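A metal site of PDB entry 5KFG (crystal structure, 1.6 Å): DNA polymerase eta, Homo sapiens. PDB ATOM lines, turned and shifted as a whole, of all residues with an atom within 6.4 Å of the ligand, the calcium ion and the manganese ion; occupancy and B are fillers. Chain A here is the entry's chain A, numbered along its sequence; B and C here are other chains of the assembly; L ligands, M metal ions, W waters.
The calcium ion is bound by OD1 of Asp 16. O of Met 17 is bound to the calcium ion, 2.2 Å away. OD2 of Asp 118 is bound to the calcium ion, at 2.3 Å. O1 of the ligand is bound to the calcium ion. An oxygen (O4) of the ligand binds the calcium ion, 2.4 Å away. An oxygen (O7) of the ligand is bound to the calcium ion (2.4 Å).
The manganese ion is bound by OE2 of Glu 119, water W1, OD1 of Asp 118, O3' of DT 8 of chain B and O7 of the ligand. The manganese ion has five donor atoms within binding distance. Slightly farther from the manganese ion lies the side-chain carboxylate (OD2) of Asp 16 (2.7 Å). Slightly farther from the manganese ion lies OD1 of Asp 16 (2.9 Å).
Within 4 Å of the calcium ion: Asp 16, Met 17 and Asp 118. The nearest printed residue that does not touch the calcium ion is Cys 19 (4.4 Å).
N of Cys 19 lies within hydrogen-bond range of O2 of the ligand, at 2.9 Å. The side-chain hydroxyl (OH) of Tyr 55 is in hydrogen-bond range of an oxygen (O2) of the ligand (2.6 Å). O4 of DT 4 of chain C is in hydrogen-bond range of a nitrogen (N3) of the ligand (3.0 Å). The side-chain amino group (NZ) of Lys 234 lies within salt-bridge range of an oxygen (O3) of the ligand, at 2.6 Å. The backbone NH (N) of Phe 21 lies within hydrogen-bond range of an oxygen (O12) of the ligand, 3.1 Å away. NH1 of Arg 58 is in salt-bridge range of O3 of the ligand (3.0 Å). N3 of DT 8 of chain B is in hydrogen-bond range of N3 of the ligand (3.5 Å). O5 of the ligand is in salt-bridge range of NH2 of Arg 64 (3.1 Å). An oxygen (O12) of the ligand sits at hydrogen-bond distance from the backbone NH (N) of Phe 20, 3.5 Å away.
OD1 of Asp 18 lies within hydrogen-bond range of OG of Ser 216, 2.9 Å away. The backbone NH (N) of Glu 119 sits at hydrogen-bond distance from the side-chain hydroxyl (OG) of Ser 116, 3.3 Å away. NE of Arg 58 is in hydrogen-bond range of O of Val 53 (2.9 Å). O2 of DT 4 of chain C sits at hydrogen-bond distance from the side-chain amide nitrogen of Gln 41. The guanidinium group (NE) of Arg 64 is in hydrogen-bond range of the backbone carbonyl oxygen (O) of Ile 51 (2.9 Å). The side-chain amino group (NZ) of Lys 227 lies within salt-bridge range of OP1 of DT 8 of chain B (3.9 Å). NZ of Lys 227 is in salt-bridge range of OD2 of Asp 16 (3.0 Å). O3' of DT 8 of chain B lies close to the side-chain hydroxyl (OG) of Ser 116, 3.5 Å away.
Residues that only touch the manganese ion: Ser 116 (3.8 Å). Within 4 Å of the manganese ion: Asp 16, Ser 116, Asp 118, Glu 119 and DT 8 of chain B.
N1 of DA 5 of chain C sits close to N4 of the ligand, 3.4 Å away. CA of Asp 18 touches O2 of the ligand, 3.5 Å away. Ile 51 touches the ligand. Ala 52 touches the ligand (CB to O12, 3.5 Å). Ile 117 touches the ligand (CG2 to O11, 3.8 Å). Hydrophobic or aromatic side chains that line the ligand: Phe 20, Phe 21, Ile 51, Ala 52, Tyr 55 and Ile 117. Of the 27 residues printed, 17 come within 4 Å of the ligand. The nearest printed residue that does not touch the ligand is Glu 119 (4.4 Å).
Water W1 lies within hydrogen-bond range of OD2 of Asp 16 (2.7 Å) and NZ of Lys 227 (2.9 Å). Water W6 lies within hydrogen-bond range of O11 of the ligand and OG of Ser 116. Water W2 bridges O2 of DT 8 of chain B (2.6 Å) and O11 of the ligand (3.4 Å).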
ATOM      1  N   ASP A  16     -14.699  13.101  14.944  1.00  0.00           N
ATOM      2  CA  ASP A  16     -15.968  13.780  14.713  1.00  0.00           C
ATOM      3  C   ASP A  16     -17.127  12.811  14.947  1.00  0.00           C
ATOM      4  O   ASP A  16     -17.182  11.765  14.314  1.00  0.00           O
ATOM      5  CB  ASP A  16     -15.998  14.304  13.273  1.00  0.00           C
ATOM      6  CG  ASP A  16     -16.947  15.471  13.092  1.00  0.00           C
ATOM      7  OD1 ASP A  16     -18.159  15.275  13.279  1.00  0.00           O
ATOM      8  OD2 ASP A  16     -16.476  16.578  12.740  1.00  0.00           O
ATOM      9  N   MET A  17     -18.063  13.153  15.829  1.00  0.00           N
ATOM     10  CA  MET A  17     -19.132  12.201  16.134  1.00  0.00           C
ATOM     11  C   MET A  17     -20.082  12.022  14.944  1.00  0.00           C
ATOM     12  O   MET A  17     -20.334  12.974  14.229  1.00  0.00           O
ATOM     13  CB  MET A  17     -19.914  12.655  17.363  1.00  0.00           C
ATOM     14  CG  MET A  17     -19.058  12.966  18.568  1.00  0.00           C
ATOM     15  SD  MET A  17     -17.991  11.608  19.067  1.00  0.00           S
ATOM     16  CE  MET A  17     -19.177  10.377  19.463  1.00  0.00           C
ATOM     17  N   ASP A  18     -20.587  10.815  14.729  1.00  0.00           N
ATOM     18  CA  ASP A  18     -21.556  10.601  13.648  1.00  0.00           C
ATOM     19  C   ASP A  18     -22.935  11.123  14.039  1.00  0.00           C
ATOM     20  O   ASP A  18     -23.416  10.795  15.139  1.00  0.00           O
ATOM     21  CB  ASP A  18     -21.716   9.117  13.313  1.00  0.00           C
ATOM     22  CG  ASP A  18     -20.422   8.470  12.840  1.00  0.00           C
ATOM     23  OD1 ASP A  18     -19.577   9.176  12.258  1.00  0.00           O
ATOM     24  OD2 ASP A  18     -20.277   7.249  13.032  1.00  0.00           O
ATOM     25  N   CYS A  19     -23.535  11.920  13.155  1.00  0.00           N
ATOM     26  CA  CYS A  19     -24.888  12.498  13.340  1.00  0.00           C
ATOM     27  C   CYS A  19     -25.174  12.751  14.821  1.00  0.00           C
ATOM     28  O   CYS A  19     -26.073  12.142  15.413  1.00  0.00           O
ATOM     29  CB  CYS A  19     -25.988  11.639  12.704  1.00  0.00           C
ATOM     30  SG  CYS A  19     -26.047   9.883  13.114  1.00  0.00           S
ATOM     31  N   PHE A  20     -24.385  13.632  15.425  1.00  0.00           N
ATOM     32  CA  PHE A  20     -24.203  13.629  16.883  1.00  0.00           C
ATOM     33  C   PHE A  20     -25.499  13.809  17.679  1.00  0.00           C
ATOM     34  O   PHE A  20     -25.796  12.970  18.534  1.00  0.00           O
ATOM     35  CB  PHE A  20     -23.200  14.717  17.301  1.00  0.00           C
ATOM     36  CG  PHE A  20     -22.900  14.725  18.775  1.00  0.00           C
ATOM     37  CD1 PHE A  20     -22.597  13.556  19.451  1.00  0.00           C
ATOM     38  CD2 PHE A  20     -22.940  15.910  19.496  1.00  0.00           C
ATOM     39  CE1 PHE A  20     -22.326  13.565  20.821  1.00  0.00           C
ATOM     40  CE2 PHE A  20     -22.657  15.926  20.869  1.00  0.00           C
ATOM     41  CZ  PHE A  20     -22.350  14.759  21.517  1.00  0.00           C
ATOM     42  N   PHE A  21     -26.284  14.857  17.407  1.00  0.00           N
ATOM     43  CA  PHE A  21     -27.471  15.063  18.234  1.00  0.00           C
ATOM     44  C   PHE A  21     -28.443  13.890  18.077  1.00  0.00           C
ATOM     45  O   PHE A  21     -29.156  13.550  19.016  1.00  0.00           O
ATOM     46  CB  PHE A  21     -28.206  16.369  17.910  1.00  0.00           C
ATOM     47  CG  PHE A  21     -27.496  17.619  18.321  1.00  0.00           C
ATOM     48  CD1 PHE A  21     -26.165  17.635  18.719  1.00  0.00           C
ATOM     49  CD2 PHE A  21     -28.184  18.823  18.300  1.00  0.00           C
ATOM     50  CE1 PHE A  21     -25.543  18.835  19.091  1.00  0.00           C
ATOM     51  CE2 PHE A  21     -27.570  20.019  18.678  1.00  0.00           C
ATOM     52  CZ  PHE A  21     -26.251  20.020  19.052  1.00  0.00           C
ATOM     53  N   VAL A  22     -28.496  13.300  16.889  1.00  0.00           N
ATOM     54  CA  VAL A  22     -29.330  12.116  16.691  1.00  0.00           C
ATOM     55  C   VAL A  22     -28.864  10.957  17.577  1.00  0.00           C
ATOM     56  O   VAL A  22     -29.680  10.285  18.217  1.00  0.00           O
ATOM     57  CB  VAL A  22     -29.336  11.694  15.205  1.00  0.00           C
ATOM     58  CG1 VAL A  22     -29.833  10.245  15.038  1.00  0.00           C
ATOM     59  CG2 VAL A  22     -30.183  12.683  14.374  1.00  0.00           C
ATOM     60  N   GLN A  41     -35.755  21.564  16.021  1.00  0.00           N
ATOM     61  CA  GLN A  41     -36.039  22.556  17.057  1.00  0.00           C
ATOM     62  C   GLN A  41     -37.246  23.370  16.662  1.00  0.00           C
ATOM     63  O   GLN A  41     -37.425  23.746  15.509  1.00  0.00           O
ATOM     64  CB  GLN A  41     -34.829  23.435  17.379  1.00  0.00           C
ATOM     65  CG  GLN A  41     -34.174  24.154  16.243  1.00  0.00           C
ATOM     66  CD  GLN A  41     -32.813  24.748  16.626  1.00  0.00           C
ATOM     67  OE1 GLN A  41     -32.300  24.550  17.741  1.00  0.00           O
ATOM     68  NE2 GLN A  41     -32.228  25.469  15.696  1.00  0.00           N
ATOM     69  N   ILE A  51     -31.929  19.933  12.535  1.00  0.00           N
ATOM     70  CA  ILE A  51     -30.539  20.281  12.768  1.00  0.00           C
ATOM     71  C   ILE A  51     -29.596  19.075  12.779  1.00  0.00           C
ATOM     72  O   ILE A  51     -28.395  19.258  12.776  1.00  0.00           O
ATOM     73  CB  ILE A  51     -30.345  21.086  14.076  1.00  0.00           C
ATOM     74  CG1 ILE A  51     -30.808  20.319  15.318  1.00  0.00           C
ATOM     75  CG2 ILE A  51     -31.038  22.457  13.964  1.00  0.00           C
ATOM     76  CD1 ILE A  51     -30.453  21.043  16.638  1.00  0.00           C
ATOM     77  N   ALA A  52     -30.142  17.862  12.766  1.00  0.00           N
ATOM     78  CA  ALA A  52     -29.306  16.654  12.676  1.00  0.00           C
ATOM     79  C   ALA A  52     -30.123  15.517  12.084  1.00  0.00           C
ATOM     80  O   ALA A  52     -31.325  15.455  12.315  1.00  0.00           O
ATOM     81  CB  ALA A  52     -28.743  16.258  14.057  1.00  0.00           C
ATOM     82  N   VAL A  53     -29.482  14.647  11.295  1.00  0.00           N
ATOM     83  CA  VAL A  53     -30.171  13.622  10.502  1.00  0.00           C
ATOM     84  C   VAL A  53     -29.437  12.295  10.537  1.00  0.00           C
ATOM     85  O   VAL A  53     -28.223  12.255  10.240  1.00  0.00           O
ATOM     86  CB  VAL A  53     -30.285  14.055   9.020  1.00  0.00           C
ATOM     87  CG1 VAL A  53     -31.151  13.092   8.217  1.00  0.00           C
ATOM     88  CG2 VAL A  53     -30.832  15.473   8.897  1.00  0.00           C
ATOM     89  N   TYR A  55     -28.219   8.557   9.313  1.00  0.00           N
ATOM     90  CA  TYR A  55     -27.801   8.126   7.989  1.00  0.00           C
ATOM     91  C   TYR A  55     -28.915   7.386   7.256  1.00  0.00           C
ATOM     92  O   TYR A  55     -29.018   7.503   6.036  1.00  0.00           O
ATOM     93  CB  TYR A  55     -26.526   7.279   8.088  1.00  0.00           C
ATOM     94  CG  TYR A  55     -25.334   8.190   8.254  1.00  0.00           C
ATOM     95  CD1 TYR A  55     -25.013   8.725   9.499  1.00  0.00           C
ATOM     96  CD2 TYR A  55     -24.571   8.582   7.169  1.00  0.00           C
ATOM     97  CE1 TYR A  55     -23.962   9.604   9.658  1.00  0.00           C
ATOM     98  CE2 TYR A  55     -23.501   9.459   7.315  1.00  0.00           C
ATOM     99  CZ  TYR A  55     -23.197   9.965   8.555  1.00  0.00           C
ATOM    100  OH  TYR A  55     -22.137  10.848   8.694  1.00  0.00           O
ATOM    101  N   ARG A  58     -30.887  10.190   5.745  1.00  0.00           N
ATOM    102  CA  ARG A  58     -30.170  10.859   4.654  1.00  0.00           C
ATOM    103  C   ARG A  58     -30.385  10.123   3.330  1.00  0.00           C
ATOM    104  O   ARG A  58     -30.371  10.751   2.265  1.00  0.00           O
ATOM    105  CB  ARG A  58     -28.686  10.939   4.957  1.00  0.00           C
ATOM    106  CG  ARG A  58     -28.381  11.767   6.160  1.00  0.00           C
ATOM    107  CD  ARG A  58     -26.899  11.860   6.399  1.00  0.00           C
ATOM    108  NE  ARG A  58     -26.662  12.340   7.764  1.00  0.00           N
ATOM    109  CZ  ARG A  58     -25.509  12.766   8.247  1.00  0.00           C
ATOM    110  NH1 ARG A  58     -24.435  12.826   7.461  1.00  0.00           N
ATOM    111  NH2 ARG A  58     -25.435  13.175   9.518  1.00  0.00           N
ATOM    112  N   ARG A  64     -30.049  18.683   6.935  1.00  0.00           N
ATOM    113  CA  ARG A  64     -30.091  19.805   7.822  1.00  0.00           C
ATOM    114  C   ARG A  64     -30.659  21.039   7.146  1.00  0.00           C
ATOM    115  O   ARG A  64     -30.527  21.207   5.977  1.00  0.00           O
ATOM    116  CB  ARG A  64     -28.667  20.056   8.379  1.00  0.00           C
ATOM    117  CG  ARG A  64     -28.436  21.274   9.218  1.00  0.00           C
ATOM    118  CD  ARG A  64     -26.973  21.296   9.613  1.00  0.00           C
ATOM    119  NE  ARG A  64     -26.746  20.255  10.565  1.00  0.00           N
ATOM    120  CZ  ARG A  64     -25.717  19.418  10.605  1.00  0.00           C
ATOM    121  NH1 ARG A  64     -24.665  19.502   9.790  1.00  0.00           N
ATOM    122  NH2 ARG A  64     -25.762  18.539  11.560  1.00  0.00           N
ATOM    123  N   LEU A  92     -29.713  23.716  24.566  1.00  0.00           N
ATOM    124  CA  LEU A  92     -28.847  22.653  24.023  1.00  0.00           C
ATOM    125  C   LEU A  92     -28.030  21.926  25.100  1.00  0.00           C
ATOM    126  O   LEU A  92     -27.062  21.242  24.782  1.00  0.00           O
ATOM    127  CB  LEU A  92     -27.915  23.232  22.972  1.00  0.00           C
ATOM    128  CG  LEU A  92     -28.606  24.053  21.871  1.00  0.00           C
ATOM    129  CD1 LEU A  92     -27.569  24.718  20.987  1.00  0.00           C
ATOM    130  CD2 LEU A  92     -29.511  23.128  21.061  1.00  0.00           C
ATOM    131  N   SER A 116     -15.523  21.919  17.987  1.00  0.00           N
ATOM    132  CA  SER A 116     -16.961  22.126  17.921  1.00  0.00           C
ATOM    133  C   SER A 116     -17.613  21.300  19.011  1.00  0.00           C
ATOM    134  O   SER A 116     -16.930  20.602  19.751  1.00  0.00           O
ATOM    135  CB  SER A 116     -17.533  21.722  16.563  1.00  0.00           C
ATOM    136  OG  SER A 116     -17.761  20.327  16.509  1.00  0.00           O
ATOM    137  N   ILE A 117     -18.938  21.343  19.086  1.00  0.00           N
ATOM    138  CA  ILE A 117     -19.635  20.566  20.082  1.00  0.00           C
ATOM    139  C   ILE A 117     -19.389  19.056  19.876  1.00  0.00           C
ATOM    140  O   ILE A 117     -19.506  18.286  20.826  1.00  0.00           O
ATOM    141  CB  ILE A 117     -21.164  20.882  20.073  1.00  0.00           C
ATOM    142  CG1 ILE A 117     -21.824  20.418  21.379  1.00  0.00           C
ATOM    143  CG2 ILE A 117     -21.826  20.265  18.832  1.00  0.00           C
ATOM    144  CD1 ILE A 117     -23.241  20.965  21.567  1.00  0.00           C
ATOM    145  N   ASP A 118     -19.048  18.629  18.664  1.00  0.00           N
ATOM    146  CA  ASP A 118     -18.926  17.182  18.463  1.00  0.00           C
ATOM    147  C   ASP A 118     -17.603  16.754  17.838  1.00  0.00           C
ATOM    148  O   ASP A 118     -17.496  15.635  17.326  1.00  0.00           O
ATOM    149  CB  ASP A 118     -20.091  16.667  17.618  1.00  0.00           C
ATOM    150  CG  ASP A 118     -19.830  16.767  16.122  1.00  0.00           C
ATOM    151  OD1 ASP A 118     -19.230  17.772  15.661  1.00  0.00           O
ATOM    152  OD2 ASP A 118     -20.187  15.793  15.413  1.00  0.00           O
ATOM    153  N   GLU A 119     -16.591  17.609  17.881  1.00  0.00           N
ATOM    154  CA  GLU A 119     -15.303  17.172  17.344  1.00  0.00           C
ATOM    155  C   GLU A 119     -14.111  17.830  17.985  1.00  0.00           C
ATOM    156  O   GLU A 119     -14.193  18.938  18.521  1.00  0.00           O
ATOM    157  CB  GLU A 119     -15.249  17.396  15.855  1.00  0.00           C
ATOM    158  CG  GLU A 119     -14.999  18.822  15.442  1.00  0.00           C
ATOM    159  CD  GLU A 119     -15.617  19.113  14.101  1.00  0.00           C
ATOM    160  OE1 GLU A 119     -14.878  19.181  13.094  1.00  0.00           O
ATOM    161  OE2 GLU A 119     -16.863  19.243  14.038  1.00  0.00           O
ATOM    162  N   SER A 216     -16.373   9.076  13.491  1.00  0.00           N
ATOM    163  CA  SER A 216     -15.408   8.899  12.423  1.00  0.00           C
ATOM    164  C   SER A 216     -14.155   9.676  12.769  1.00  0.00           C
ATOM    165  O   SER A 216     -14.180  10.496  13.676  1.00  0.00           O
ATOM    166  CB  SER A 216     -15.993   9.371  11.098  1.00  0.00           C
ATOM    167  OG  SER A 216     -17.128   8.581  10.788  1.00  0.00           O
ATOM    168  N   LYS A 227      -9.002  16.761   9.062  1.00  0.00           N
ATOM    169  CA  LYS A 227     -10.381  16.987   8.927  1.00  0.00           C
ATOM    170  C   LYS A 227     -10.953  16.528   7.570  1.00  0.00           C
ATOM    171  O   LYS A 227     -12.019  16.003   7.476  1.00  0.00           O
ATOM    172  CB  LYS A 227     -10.760  18.517   9.031  1.00  0.00           C
ATOM    173  CG  LYS A 227     -12.093  19.068   8.779  1.00  0.00           C
ATOM    174  CD  LYS A 227     -13.057  18.443   9.777  1.00  0.00           C
ATOM    175  CE  LYS A 227     -14.497  18.942   9.548  1.00  0.00           C
ATOM    176  NZ  LYS A 227     -15.487  18.384  10.521  1.00  0.00           N
ATOM    177  N   LYS A 234     -17.069   8.388   6.322  1.00  0.00           N
ATOM    178  CA  LYS A 234     -18.099   8.337   7.373  1.00  0.00           C
ATOM    179  C   LYS A 234     -19.307   7.519   6.921  1.00  0.00           C
ATOM    180  O   LYS A 234     -19.557   7.432   5.767  1.00  0.00           O
ATOM    181  CB  LYS A 234     -18.448   9.768   7.779  1.00  0.00           C
ATOM    182  CG  LYS A 234     -19.124  10.528   6.709  1.00  0.00           C
ATOM    183  CD  LYS A 234     -19.275  11.998   7.059  1.00  0.00           C
ATOM    184  CE  LYS A 234     -20.525  12.551   6.381  1.00  0.00           C
ATOM    185  NZ  LYS A 234     -20.750  13.973   6.780  1.00  0.00           N
ATOM    186  N   PRO A 235     -20.193   6.902   7.815  1.00  0.00           N
ATOM    187  CA  PRO A 235     -19.890   6.991   9.241  1.00  0.00           C
ATOM    188  C   PRO A 235     -19.151   5.806   9.851  1.00  0.00           C
ATOM    189  O   PRO A 235     -18.978   4.856   9.200  1.00  0.00           O
ATOM    190  CB  PRO A 235     -21.283   7.022   9.858  1.00  0.00           C
ATOM    191  CG  PRO A 235     -22.056   6.068   9.090  1.00  0.00           C
ATOM    192  CD  PRO A 235     -21.598   6.242   7.713  1.00  0.00           C
ATOM    193  P    DT B   8     -17.951  22.731   9.101  1.00  0.00           P
ATOM    194  OP1  DT B   8     -17.223  21.481   8.835  1.00  0.00           O
ATOM    195  OP2  DT B   8     -19.106  23.126   8.253  1.00  0.00           O
ATOM    196  O5'  DT B   8     -18.489  22.722  10.636  1.00  0.00           O
ATOM    197  C5'  DT B   8     -17.692  22.246  11.794  1.00  0.00           C
ATOM    198  C4'  DT B   8     -18.650  22.058  12.968  1.00  0.00           C
ATOM    199  O4'  DT B   8     -19.342  23.320  13.082  1.00  0.00           O
ATOM    200  C3'  DT B   8     -19.680  20.998  12.622  1.00  0.00           C
ATOM    201  O3'  DT B   8     -19.791  20.072  13.671  1.00  0.00           O
ATOM    202  C2'  DT B   8     -20.989  21.790  12.412  1.00  0.00           C
ATOM    203  C1'  DT B   8     -20.730  23.079  13.177  1.00  0.00           C
ATOM    204  N1   DT B   8     -21.473  24.228  12.591  1.00  0.00           N
ATOM    205  C2   DT B   8     -22.434  24.862  13.349  1.00  0.00           C
ATOM    206  O2   DT B   8     -22.709  24.551  14.492  1.00  0.00           O
ATOM    207  N3   DT B   8     -23.077  25.883  12.706  1.00  0.00           N
ATOM    208  C4   DT B   8     -22.861  26.328  11.419  1.00  0.00           C
ATOM    209  O4   DT B   8     -23.484  27.262  10.934  1.00  0.00           O
ATOM    210  C5   DT B   8     -21.848  25.606  10.686  1.00  0.00           C
ATOM    211  C7   DT B   8     -21.533  26.003   9.271  1.00  0.00           C
ATOM    212  C6   DT B   8     -21.216  24.604  11.295  1.00  0.00           C
ATOM    213  P    DT C   3     -36.053  30.625   5.722  1.00  0.00           P
ATOM    214  OP1  DT C   3     -35.548  31.939   5.267  1.00  0.00           O
ATOM    215  OP2  DT C   3     -36.763  29.718   4.788  1.00  0.00           O
ATOM    216  O5'  DT C   3     -34.830  29.818   6.364  1.00  0.00           O
ATOM    217  C5'  DT C   3     -35.071  28.698   7.182  1.00  0.00           C
ATOM    218  C4'  DT C   3     -33.847  28.370   8.003  1.00  0.00           C
ATOM    219  O4'  DT C   3     -32.902  27.654   7.191  1.00  0.00           O
ATOM    220  C3'  DT C   3     -33.112  29.604   8.538  1.00  0.00           C
ATOM    221  O3'  DT C   3     -33.026  29.547   9.962  1.00  0.00           O
ATOM    222  C2'  DT C   3     -31.736  29.545   7.865  1.00  0.00           C
ATOM    223  C1'  DT C   3     -31.600  28.079   7.499  1.00  0.00           C
ATOM    224  N1   DT C   3     -30.748  27.833   6.316  1.00  0.00           N
ATOM    225  C2   DT C   3     -29.669  26.994   6.433  1.00  0.00           C
ATOM    226  O2   DT C   3     -29.365  26.438   7.475  1.00  0.00           O
ATOM    227  N3   DT C   3     -28.945  26.841   5.285  1.00  0.00           N
ATOM    228  C4   DT C   3     -29.188  27.422   4.060  1.00  0.00           C
ATOM    229  O4   DT C   3     -28.475  27.213   3.070  1.00  0.00           O
ATOM    230  C5   DT C   3     -30.333  28.295   4.002  1.00  0.00           C
ATOM    231  C7   DT C   3     -30.703  28.985   2.722  1.00  0.00           C
ATOM    232  C6   DT C   3     -31.053  28.451   5.122  1.00  0.00           C
ATOM    233  P    DT C   4     -33.749  30.685  10.834  1.00  0.00           P
ATOM    234  OP1  DT C   4     -35.186  30.695  10.475  1.00  0.00           O
ATOM    235  OP2  DT C   4     -32.927  31.902  10.661  1.00  0.00           O
ATOM    236  O5'  DT C   4     -33.546  30.215  12.352  1.00  0.00           O
ATOM    237  C5'  DT C   4     -34.518  29.402  13.036  1.00  0.00           C
ATOM    238  C4'  DT C   4     -33.894  28.829  14.312  1.00  0.00           C
ATOM    239  O4'  DT C   4     -32.783  27.984  13.917  1.00  0.00           O
ATOM    240  C3'  DT C   4     -33.297  29.882  15.247  1.00  0.00           C
ATOM    241  O3'  DT C   4     -33.423  29.411  16.579  1.00  0.00           O
ATOM    242  C2'  DT C   4     -31.838  29.951  14.792  1.00  0.00           C
ATOM    243  C1'  DT C   4     -31.582  28.484  14.470  1.00  0.00           C
ATOM    244  N1   DT C   4     -30.510  28.209  13.492  1.00  0.00           N
ATOM    245  C2   DT C   4     -29.759  27.103  13.703  1.00  0.00           C
ATOM    246  O2   DT C   4     -29.893  26.390  14.686  1.00  0.00           O
ATOM    247  N3   DT C   4     -28.809  26.858  12.762  1.00  0.00           N
ATOM    248  C4   DT C   4     -28.551  27.580  11.631  1.00  0.00           C
ATOM    249  O4   DT C   4     -27.667  27.265  10.839  1.00  0.00           O
ATOM    250  C5   DT C   4     -29.394  28.742  11.442  1.00  0.00           C
ATOM    251  C7   DT C   4     -29.208  29.632  10.241  1.00  0.00           C
ATOM    252  C6   DT C   4     -30.342  28.988  12.370  1.00  0.00           C
ATOM    253  P    DA C   5     -32.922  30.295  17.820  1.00  0.00           P
ATOM    254  OP1  DA C   5     -33.914  30.117  18.890  1.00  0.00           O
ATOM    255  OP2  DA C   5     -32.550  31.648  17.344  1.00  0.00           O
ATOM    256  O5'  DA C   5     -31.563  29.583  18.245  1.00  0.00           O
ATOM    257  C5'  DA C   5     -31.593  28.255  18.768  1.00  0.00           C
ATOM    258  C4'  DA C   5     -30.206  27.832  19.185  1.00  0.00           C
ATOM    259  O4'  DA C   5     -29.379  27.607  18.000  1.00  0.00           O
ATOM    260  C3'  DA C   5     -29.454  28.863  20.008  1.00  0.00           C
ATOM    261  O3'  DA C   5     -28.674  28.188  20.986  1.00  0.00           O
ATOM    262  C2'  DA C   5     -28.566  29.564  18.979  1.00  0.00           C
ATOM    263  C1'  DA C   5     -28.193  28.363  18.113  1.00  0.00           C
ATOM    264  N9   DA C   5     -27.736  28.713  16.776  1.00  0.00           N
ATOM    265  C8   DA C   5     -28.188  29.719  15.984  1.00  0.00           C
ATOM    266  N7   DA C   5     -27.599  29.768  14.811  1.00  0.00           N
ATOM    267  C5   DA C   5     -26.714  28.700  14.836  1.00  0.00           C
ATOM    268  C6   DA C   5     -25.781  28.215  13.896  1.00  0.00           C
ATOM    269  N6   DA C   5     -25.606  28.769  12.694  1.00  0.00           N
ATOM    270  N1   DA C   5     -25.050  27.138  14.236  1.00  0.00           N
ATOM    271  C2   DA C   5     -25.243  26.586  15.451  1.00  0.00           C
ATOM    272  N3   DA C   5     -26.083  26.958  16.420  1.00  0.00           N
ATOM    273  C4   DA C   5     -26.791  28.037  16.039  1.00  0.00           C
HETATM  274  P1  LIG L   1     -22.137  13.938  10.446  1.00  0.00           P
HETATM  275  O1  LIG L   1     -20.932  14.615  11.047  1.00  0.00           O
HETATM  276  O2  LIG L   1     -22.185  12.459  10.700  1.00  0.00           O
HETATM  277  O3  LIG L   1     -22.243  14.220   8.949  1.00  0.00           O
HETATM  278  P2  LIG L   1     -23.538  15.621  12.304  1.00  0.00           P
HETATM  279  O4  LIG L   1     -22.702  15.130  13.466  1.00  0.00           O
HETATM  280  O5  LIG L   1     -25.001  15.796  12.683  1.00  0.00           O
HETATM  281  O6  LIG L   1     -23.473  14.558  11.089  1.00  0.00           O
HETATM  282  P3  LIG L   1     -21.920  18.019  12.280  1.00  0.00           P
HETATM  283  O7  LIG L   1     -20.631  17.343  12.657  1.00  0.00           O
HETATM  284  O8  LIG L   1     -21.770  19.054  11.176  1.00  0.00           O
HETATM  285  O9  LIG L   1     -23.006  16.988  11.693  1.00  0.00           O
HETATM  286  O10 LIG L   1     -22.600  18.752  13.502  1.00  0.00           O
HETATM  287  C1  LIG L   1     -22.629  18.163  14.777  1.00  0.00           C
HETATM  288  C2  LIG L   1     -23.901  18.588  15.516  1.00  0.00           C
HETATM  289  O11 LIG L   1     -23.899  19.995  15.657  1.00  0.00           O
HETATM  290  C3  LIG L   1     -25.094  18.209  14.789  1.00  0.00           C
HETATM  291  O12 LIG L   1     -25.526  16.888  15.160  1.00  0.00           O
HETATM  292  C4  LIG L   1     -26.081  19.234  15.177  1.00  0.00           C
HETATM  293  C5  LIG L   1     -25.238  20.454  15.408  1.00  0.00           C
HETATM  294  N1  LIG L   1     -25.221  21.340  14.285  1.00  0.00           N
HETATM  295  C6  LIG L   1     -24.446  21.264  13.181  1.00  0.00           C
HETATM  296  N2  LIG L   1     -24.724  22.253  12.338  1.00  0.00           N
HETATM  297  C7  LIG L   1     -25.671  23.025  12.890  1.00  0.00           C
HETATM  298  C8  LIG L   1     -26.347  24.173  12.507  1.00  0.00           C
HETATM  299  N3  LIG L   1     -26.044  24.789  11.264  1.00  0.00           N
HETATM  300  N4  LIG L   1     -27.278  24.687  13.314  1.00  0.00           N
HETATM  301  C9  LIG L   1     -27.581  24.139  14.515  1.00  0.00           C
HETATM  302  N5  LIG L   1     -26.946  23.004  14.923  1.00  0.00           N
HETATM  303  C10 LIG L   1     -26.008  22.448  14.134  1.00  0.00           C
HETATM  304 CA    CA M   1     -20.354  15.005  13.293  1.00  0.00          CA
HETATM  305 MN    MN M   2     -18.577  18.092  13.571  1.00  0.00          MN
HETATM  306  O   HOH W   1     -18.254  18.204  11.438  1.00  0.00           O
HETATM  307  O   HOH W   2     -23.368  23.212  16.624  1.00  0.00           O
HETATM  308  O   HOH W   3     -23.890  22.979   9.698  1.00  0.00           O
HETATM  309  O   HOH W   4     -19.418  16.262   9.691  1.00  0.00           O
HETATM  310  O   HOH W   5     -27.270  23.160  17.700  1.00  0.00           O
HETATM  311  O   HOH W   6     -21.042  21.082  15.621  1.00  0.00           O
HETATM  312  O   HOH W   7     -26.831  15.392  10.824  1.00  0.00           O
HETATM  313  O   HOH W   8     -23.456  16.339   7.938  1.00  0.00           O
